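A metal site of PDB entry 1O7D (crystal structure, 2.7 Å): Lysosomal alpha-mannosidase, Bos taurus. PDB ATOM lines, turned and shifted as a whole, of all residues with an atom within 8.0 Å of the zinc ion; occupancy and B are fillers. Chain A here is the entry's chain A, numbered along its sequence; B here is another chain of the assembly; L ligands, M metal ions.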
ATOM      1  N   HIS A  23       7.419   3.082 -24.494  1.00  0.00           N
ATOM      2  CA  HIS A  23       8.646   2.816 -25.217  1.00  0.00           C
ATOM      3  C   HIS A  23       8.966   1.336 -25.127  1.00  0.00           C
ATOM      4  O   HIS A  23       9.408   0.860 -24.088  1.00  0.00           O
ATOM      5  CB  HIS A  23       9.794   3.623 -24.617  1.00  0.00           C
ATOM      6  CG  HIS A  23      11.087   3.481 -25.355  1.00  0.00           C
ATOM      7  ND1 HIS A  23      11.227   3.856 -26.664  1.00  0.00           N
ATOM      8  CD2 HIS A  23      12.306   3.064 -24.937  1.00  0.00           C
ATOM      9  CE1 HIS A  23      12.489   3.670 -27.033  1.00  0.00           C
ATOM     10  NE2 HIS A  23      13.158   3.199 -25.998  1.00  0.00           N
ATOM     11  N   ASP A  24       8.734   0.601 -26.212  1.00  0.00           N
ATOM     12  CA  ASP A  24       8.997  -0.839 -26.255  1.00  0.00           C
ATOM     13  C   ASP A  24      10.241  -1.169 -27.088  1.00  0.00           C
ATOM     14  O   ASP A  24      10.207  -1.165 -28.312  1.00  0.00           O
ATOM     15  CB  ASP A  24       7.790  -1.573 -26.846  1.00  0.00           C
ATOM     16  CG  ASP A  24       6.544  -1.369 -26.023  1.00  0.00           C
ATOM     17  OD1 ASP A  24       6.649  -0.778 -24.921  1.00  0.00           O
ATOM     18  OD2 ASP A  24       5.454  -1.806 -26.463  1.00  0.00           O
ATOM     19  N   ASP A  25      11.336  -1.469 -26.399  1.00  0.00           N
ATOM     20  CA  ASP A  25      12.568  -1.765 -27.095  1.00  0.00           C
ATOM     21  C   ASP A  25      12.507  -3.124 -27.786  1.00  0.00           C
ATOM     22  O   ASP A  25      12.251  -4.142 -27.148  1.00  0.00           O
ATOM     23  CB  ASP A  25      13.738  -1.712 -26.104  1.00  0.00           C
ATOM     24  CG  ASP A  25      14.007  -0.309 -25.592  1.00  0.00           C
ATOM     25  OD1 ASP A  25      14.302   0.561 -26.427  1.00  0.00           O
ATOM     26  OD2 ASP A  25      13.931  -0.060 -24.370  1.00  0.00           O
ATOM     27  N   VAL A  26      12.725  -3.126 -29.094  1.00  0.00           N
ATOM     28  CA  VAL A  26      12.718  -4.381 -29.841  1.00  0.00           C
ATOM     29  C   VAL A  26      14.067  -5.041 -29.529  1.00  0.00           C
ATOM     30  O   VAL A  26      14.990  -5.097 -30.364  1.00  0.00           O
ATOM     31  CB  VAL A  26      12.559  -4.134 -31.367  1.00  0.00           C
ATOM     32  CG1 VAL A  26      12.750  -5.436 -32.135  1.00  0.00           C
ATOM     33  CG2 VAL A  26      11.162  -3.567 -31.651  1.00  0.00           C
ATOM     34  N   GLY A  27      14.168  -5.542 -28.301  1.00  0.00           N
ATOM     35  CA  GLY A  27      15.377  -6.173 -27.835  1.00  0.00           C
ATOM     36  C   GLY A  27      16.287  -5.172 -27.132  1.00  0.00           C
ATOM     37  O   GLY A  27      16.435  -4.022 -27.561  1.00  0.00           O
ATOM     38  N   TRP A  28      16.853  -5.612 -26.021  1.00  0.00           N
ATOM     39  CA  TRP A  28      17.790  -4.820 -25.233  1.00  0.00           C
ATOM     40  C   TRP A  28      18.364  -5.698 -24.130  1.00  0.00           C
ATOM     41  O   TRP A  28      19.562  -6.024 -24.144  1.00  0.00           O
ATOM     42  CB  TRP A  28      17.127  -3.586 -24.624  1.00  0.00           C
ATOM     43  CG  TRP A  28      18.074  -2.793 -23.776  1.00  0.00           C
ATOM     44  CD1 TRP A  28      19.371  -2.516 -24.071  1.00  0.00           C
ATOM     45  CD2 TRP A  28      17.811  -2.200 -22.516  1.00  0.00           C
ATOM     46  NE1 TRP A  28      19.945  -1.797 -23.065  1.00  0.00           N
ATOM     47  CE2 TRP A  28      19.006  -1.590 -22.092  1.00  0.00           C
ATOM     48  CE3 TRP A  28      16.683  -2.129 -21.691  1.00  0.00           C
ATOM     49  CZ2 TRP A  28      19.105  -0.904 -20.873  1.00  0.00           C
ATOM     50  CZ3 TRP A  28      16.779  -1.448 -20.488  1.00  0.00           C
ATOM     51  CH2 TRP A  28      17.990  -0.858 -20.090  1.00  0.00           C
ATOM     52  N   GLU A  71       6.470   0.945 -32.101  1.00  0.00           N
ATOM     53  CA  GLU A  71       7.192  -0.177 -32.696  1.00  0.00           C
ATOM     54  C   GLU A  71       6.307  -1.123 -33.511  1.00  0.00           C
ATOM     55  O   GLU A  71       5.596  -1.970 -32.973  1.00  0.00           O
ATOM     56  CB  GLU A  71       7.952  -0.953 -31.616  1.00  0.00           C
ATOM     57  CG  GLU A  71       9.064  -0.168 -30.883  1.00  0.00           C
ATOM     58  CD  GLU A  71       8.526   0.886 -29.906  1.00  0.00           C
ATOM     59  OE1 GLU A  71       7.449   0.648 -29.334  1.00  0.00           O
ATOM     60  OE2 GLU A  71       9.187   1.931 -29.690  1.00  0.00           O
ATOM     61  N   MET A 108      12.476   1.559 -33.788  1.00  0.00           N
ATOM     62  CA  MET A 108      12.958   2.934 -33.663  1.00  0.00           C
ATOM     63  C   MET A 108      14.495   2.776 -33.788  1.00  0.00           C
ATOM     64  O   MET A 108      15.197   2.479 -32.804  1.00  0.00           O
ATOM     65  CB  MET A 108      12.572   3.503 -32.302  1.00  0.00           C
ATOM     66  CG  MET A 108      12.761   4.993 -32.146  1.00  0.00           C
ATOM     67  SD  MET A 108      12.837   5.430 -30.405  1.00  0.00           S
ATOM     68  CE  MET A 108      11.205   4.985 -29.855  1.00  0.00           C
ATOM     69  N   ILE A 146      12.781   8.925 -29.160  1.00  0.00           N
ATOM     70  CA  ILE A 146      12.931   9.423 -27.817  1.00  0.00           C
ATOM     71  C   ILE A 146      14.147   8.905 -27.101  1.00  0.00           C
ATOM     72  O   ILE A 146      14.608   9.521 -26.153  1.00  0.00           O
ATOM     73  CB  ILE A 146      11.690   9.063 -27.011  1.00  0.00           C
ATOM     74  CG1 ILE A 146      11.447   7.558 -27.119  1.00  0.00           C
ATOM     75  CG2 ILE A 146      10.487   9.839 -27.546  1.00  0.00           C
ATOM     76  CD1 ILE A 146      10.260   7.066 -26.340  1.00  0.00           C
ATOM     77  N   ASP A 147      14.692   7.792 -27.563  1.00  0.00           N
ATOM     78  CA  ASP A 147      15.822   7.216 -26.867  1.00  0.00           C
ATOM     79  C   ASP A 147      17.184   7.190 -27.570  1.00  0.00           C
ATOM     80  O   ASP A 147      18.197   7.118 -26.893  1.00  0.00           O
ATOM     81  CB  ASP A 147      15.456   5.809 -26.419  1.00  0.00           C
ATOM     82  CG  ASP A 147      16.172   5.414 -25.164  1.00  0.00           C
ATOM     83  OD1 ASP A 147      17.267   5.953 -24.968  1.00  0.00           O
ATOM     84  OD2 ASP A 147      15.663   4.580 -24.400  1.00  0.00           O
ATOM     85  N   PRO A 148      17.242   7.243 -28.918  1.00  0.00           N
ATOM     86  CA  PRO A 148      18.583   7.223 -29.529  1.00  0.00           C
ATOM     87  C   PRO A 148      19.550   8.204 -28.862  1.00  0.00           C
ATOM     88  O   PRO A 148      19.143   9.251 -28.366  1.00  0.00           O
ATOM     89  CB  PRO A 148      18.300   7.562 -30.977  1.00  0.00           C
ATOM     90  CG  PRO A 148      16.977   6.933 -31.197  1.00  0.00           C
ATOM     91  CD  PRO A 148      16.198   7.289 -29.948  1.00  0.00           C
ATOM     92  N   PHE A 149      20.836   7.847 -28.872  1.00  0.00           N
ATOM     93  CA  PHE A 149      21.896   8.624 -28.228  1.00  0.00           C
ATOM     94  C   PHE A 149      22.557   9.699 -29.114  1.00  0.00           C
ATOM     95  O   PHE A 149      23.730   9.593 -29.503  1.00  0.00           O
ATOM     96  CB  PHE A 149      22.952   7.637 -27.708  1.00  0.00           C
ATOM     97  CG  PHE A 149      22.404   6.265 -27.401  1.00  0.00           C
ATOM     98  CD1 PHE A 149      23.110   5.126 -27.783  1.00  0.00           C
ATOM     99  CD2 PHE A 149      21.183   6.108 -26.757  1.00  0.00           C
ATOM    100  CE1 PHE A 149      22.597   3.838 -27.542  1.00  0.00           C
ATOM    101  CE2 PHE A 149      20.668   4.830 -26.512  1.00  0.00           C
ATOM    102  CZ  PHE A 149      21.371   3.695 -26.907  1.00  0.00           C
ATOM    103  N   ARG A 171      17.027  12.621 -26.009  1.00  0.00           N
ATOM    104  CA  ARG A 171      18.435  12.804 -25.712  1.00  0.00           C
ATOM    105  C   ARG A 171      19.264  13.821 -26.516  1.00  0.00           C
ATOM    106  O   ARG A 171      19.410  13.682 -27.742  1.00  0.00           O
ATOM    107  CB  ARG A 171      19.150  11.457 -25.789  1.00  0.00           C
ATOM    108  CG  ARG A 171      18.553  10.422 -24.867  1.00  0.00           C
ATOM    109  CD  ARG A 171      19.211   9.067 -25.062  1.00  0.00           C
ATOM    110  NE  ARG A 171      18.578   8.088 -24.190  1.00  0.00           N
ATOM    111  CZ  ARG A 171      18.766   8.063 -22.875  1.00  0.00           C
ATOM    112  NH1 ARG A 171      19.570   8.951 -22.319  1.00  0.00           N
ATOM    113  NH2 ARG A 171      18.130   7.159 -22.122  1.00  0.00           N
ATOM    114  N   TYR A 212      11.631  11.504 -21.532  1.00  0.00           N
ATOM    115  CA  TYR A 212      10.396  10.930 -22.041  1.00  0.00           C
ATOM    116  C   TYR A 212       9.569  10.350 -20.902  1.00  0.00           C
ATOM    117  O   TYR A 212       8.616   9.617 -21.123  1.00  0.00           O
ATOM    118  CB  TYR A 212      10.645   9.877 -23.142  1.00  0.00           C
ATOM    119  CG  TYR A 212      11.413   8.596 -22.820  1.00  0.00           C
ATOM    120  CD1 TYR A 212      10.781   7.491 -22.250  1.00  0.00           C
ATOM    121  CD2 TYR A 212      12.751   8.463 -23.153  1.00  0.00           C
ATOM    122  CE1 TYR A 212      11.469   6.295 -22.017  1.00  0.00           C
ATOM    123  CE2 TYR A 212      13.447   7.283 -22.933  1.00  0.00           C
ATOM    124  CZ  TYR A 212      12.809   6.201 -22.368  1.00  0.00           C
ATOM    125  OH  TYR A 212      13.521   5.047 -22.151  1.00  0.00           O
ATOM    126  N   ASP A 270       9.569   3.005 -20.374  1.00  0.00           N
ATOM    127  CA  ASP A 270       9.903   1.682 -20.880  1.00  0.00           C
ATOM    128  C   ASP A 270       8.934   0.580 -20.489  1.00  0.00           C
ATOM    129  O   ASP A 270       8.869   0.173 -19.324  1.00  0.00           O
ATOM    130  CB  ASP A 270      11.308   1.256 -20.421  1.00  0.00           C
ATOM    131  CG  ASP A 270      12.385   2.133 -20.976  1.00  0.00           C
ATOM    132  OD1 ASP A 270      12.250   2.614 -22.133  1.00  0.00           O
ATOM    133  OD2 ASP A 270      13.401   2.333 -20.272  1.00  0.00           O
ATOM    134  N   PHE A 271       8.194   0.089 -21.483  1.00  0.00           N
ATOM    135  CA  PHE A 271       7.255  -1.005 -21.274  1.00  0.00           C
ATOM    136  C   PHE A 271       6.162  -0.795 -20.259  1.00  0.00           C
ATOM    137  O   PHE A 271       5.911  -1.670 -19.422  1.00  0.00           O
ATOM    138  CB  PHE A 271       8.046  -2.270 -20.930  1.00  0.00           C
ATOM    139  CG  PHE A 271       8.926  -2.751 -22.031  1.00  0.00           C
ATOM    140  CD1 PHE A 271       8.410  -3.501 -23.078  1.00  0.00           C
ATOM    141  CD2 PHE A 271      10.279  -2.427 -22.050  1.00  0.00           C
ATOM    142  CE1 PHE A 271       9.236  -3.924 -24.123  1.00  0.00           C
ATOM    143  CE2 PHE A 271      11.110  -2.847 -23.103  1.00  0.00           C
ATOM    144  CZ  PHE A 271      10.584  -3.604 -24.134  1.00  0.00           C
ATOM    145  N   HIS B  15      17.351  -1.603 -34.792  1.00  0.00           N
ATOM    146  CA  HIS B  15      16.927  -1.082 -33.490  1.00  0.00           C
ATOM    147  C   HIS B  15      18.066  -0.234 -32.889  1.00  0.00           C
ATOM    148  O   HIS B  15      19.185  -0.237 -33.405  1.00  0.00           O
ATOM    149  CB  HIS B  15      16.618  -2.254 -32.574  1.00  0.00           C
ATOM    150  CG  HIS B  15      16.154  -1.820 -31.198  1.00  0.00           C
ATOM    151  ND1 HIS B  15      14.968  -1.154 -30.991  1.00  0.00           N
ATOM    152  CD2 HIS B  15      16.743  -1.957 -29.994  1.00  0.00           C
ATOM    153  CE1 HIS B  15      14.837  -0.896 -29.698  1.00  0.00           C
ATOM    154  NE2 HIS B  15      15.891  -1.361 -29.076  1.00  0.00           N
ATOM    155  N   HIS B  16      17.783   0.454 -31.776  1.00  0.00           N
ATOM    156  CA  HIS B  16      18.820   1.287 -31.146  1.00  0.00           C
ATOM    157  C   HIS B  16      19.677   0.581 -30.099  1.00  0.00           C
ATOM    158  O   HIS B  16      20.659   1.139 -29.622  1.00  0.00           O
ATOM    159  CB  HIS B  16      18.229   2.567 -30.572  1.00  0.00           C
ATOM    160  CG  HIS B  16      17.066   2.331 -29.631  1.00  0.00           C
ATOM    161  ND1 HIS B  16      15.772   2.216 -30.066  1.00  0.00           N
ATOM    162  CD2 HIS B  16      17.040   2.270 -28.279  1.00  0.00           C
ATOM    163  CE1 HIS B  16      14.973   2.102 -29.011  1.00  0.00           C
ATOM    164  NE2 HIS B  16      15.707   2.139 -27.926  1.00  0.00           N
ATOM    165  N   ASP B  17      19.305  -0.641 -29.773  1.00  0.00           N
ATOM    166  CA  ASP B  17      20.059  -1.426 -28.817  1.00  0.00           C
ATOM    167  C   ASP B  17      20.700  -2.591 -29.536  1.00  0.00           C
ATOM    168  O   ASP B  17      21.407  -3.371 -28.904  1.00  0.00           O
ATOM    169  CB  ASP B  17      19.139  -1.999 -27.736  1.00  0.00           C
ATOM    170  CG  ASP B  17      18.520  -0.947 -26.876  1.00  0.00           C
ATOM    171  OD1 ASP B  17      19.209   0.079 -26.652  1.00  0.00           O
ATOM    172  OD2 ASP B  17      17.360  -1.136 -26.412  1.00  0.00           O
ATOM    173  N   THR B  22      24.376  -2.245 -27.879  1.00  0.00           N
ATOM    174  CA  THR B  22      24.066  -1.881 -26.513  1.00  0.00           C
ATOM    175  C   THR B  22      23.061  -2.788 -25.848  1.00  0.00           C
ATOM    176  O   THR B  22      22.336  -2.380 -24.950  1.00  0.00           O
ATOM    177  CB  THR B  22      23.574  -0.430 -26.421  1.00  0.00           C
ATOM    178  OG1 THR B  22      22.428  -0.240 -27.270  1.00  0.00           O
ATOM    179  CG2 THR B  22      24.701   0.502 -26.841  1.00  0.00           C
HETATM  180  C1  LIG L   1      18.031   2.130 -23.508  1.00  0.00           C
HETATM  181  C2  LIG L   1      19.336   1.305 -23.584  1.00  0.00           C
HETATM  182  C3  LIG L   1      18.036   3.334 -22.478  1.00  0.00           C
HETATM  183  C4  LIG L   1      16.792   1.146 -23.314  1.00  0.00           C
HETATM  184  N1  LIG L   1      17.870   2.766 -24.775  1.00  0.00           N
HETATM  185  O1  LIG L   1      20.437   2.196 -23.757  1.00  0.00           O
HETATM  186  O2  LIG L   1      19.013   4.271 -22.710  1.00  0.00           O
HETATM  187  O3  LIG L   1      15.599   1.889 -23.640  1.00  0.00           O
HETATM  188 ZN    ZN M   1      15.099   2.377 -25.787  1.00  0.00          ZN
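Of the 20 residues printed, 4 come within 4 Å of the zinc ion.
A ring nitrogen (NE2) of His 23 sits close to the side-chain carboxylate (OD2) of Asp 147, 3.3 Å away.
The backbone carbonyl oxygen (O) of His 16 of chain B sits at hydrogen-bond distance from the side-chain hydroxyl (OG1) of Thr 22 of chain B (3.3 Å).
OD1 of Asp 147 is in salt-bridge range of NE of Arg 171 (2.6 Å).
N of Phe 271 lies within hydrogen-bond range of O of His 23 (3.0 Å).
The backbone carbonyl oxygen of Met 108 lies within hydrogen-bond range of a ring nitrogen (ND1) of His 16 of chain B (2.8 Å).
The side-chain hydroxyl of Tyr 212 is in hydrogen-bond range of the side-chain carboxylate of Asp 147, at 3.1 Å.
The zinc ion is bound by the side-chain carboxylate (OD1) of Asp 25 (2.1 Å), a ring nitrogen (NE2) of His 23 (2.1 Å), a ring nitrogen (NE2) of His 16 of chain B (2.2 Å) and an oxygen (O3) of the ligand (2.3 Å).
The zinc ion has four donor atoms within binding distance.
Slightly farther from the zinc ion lies OD2 of Asp 147 (2.7 Å).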
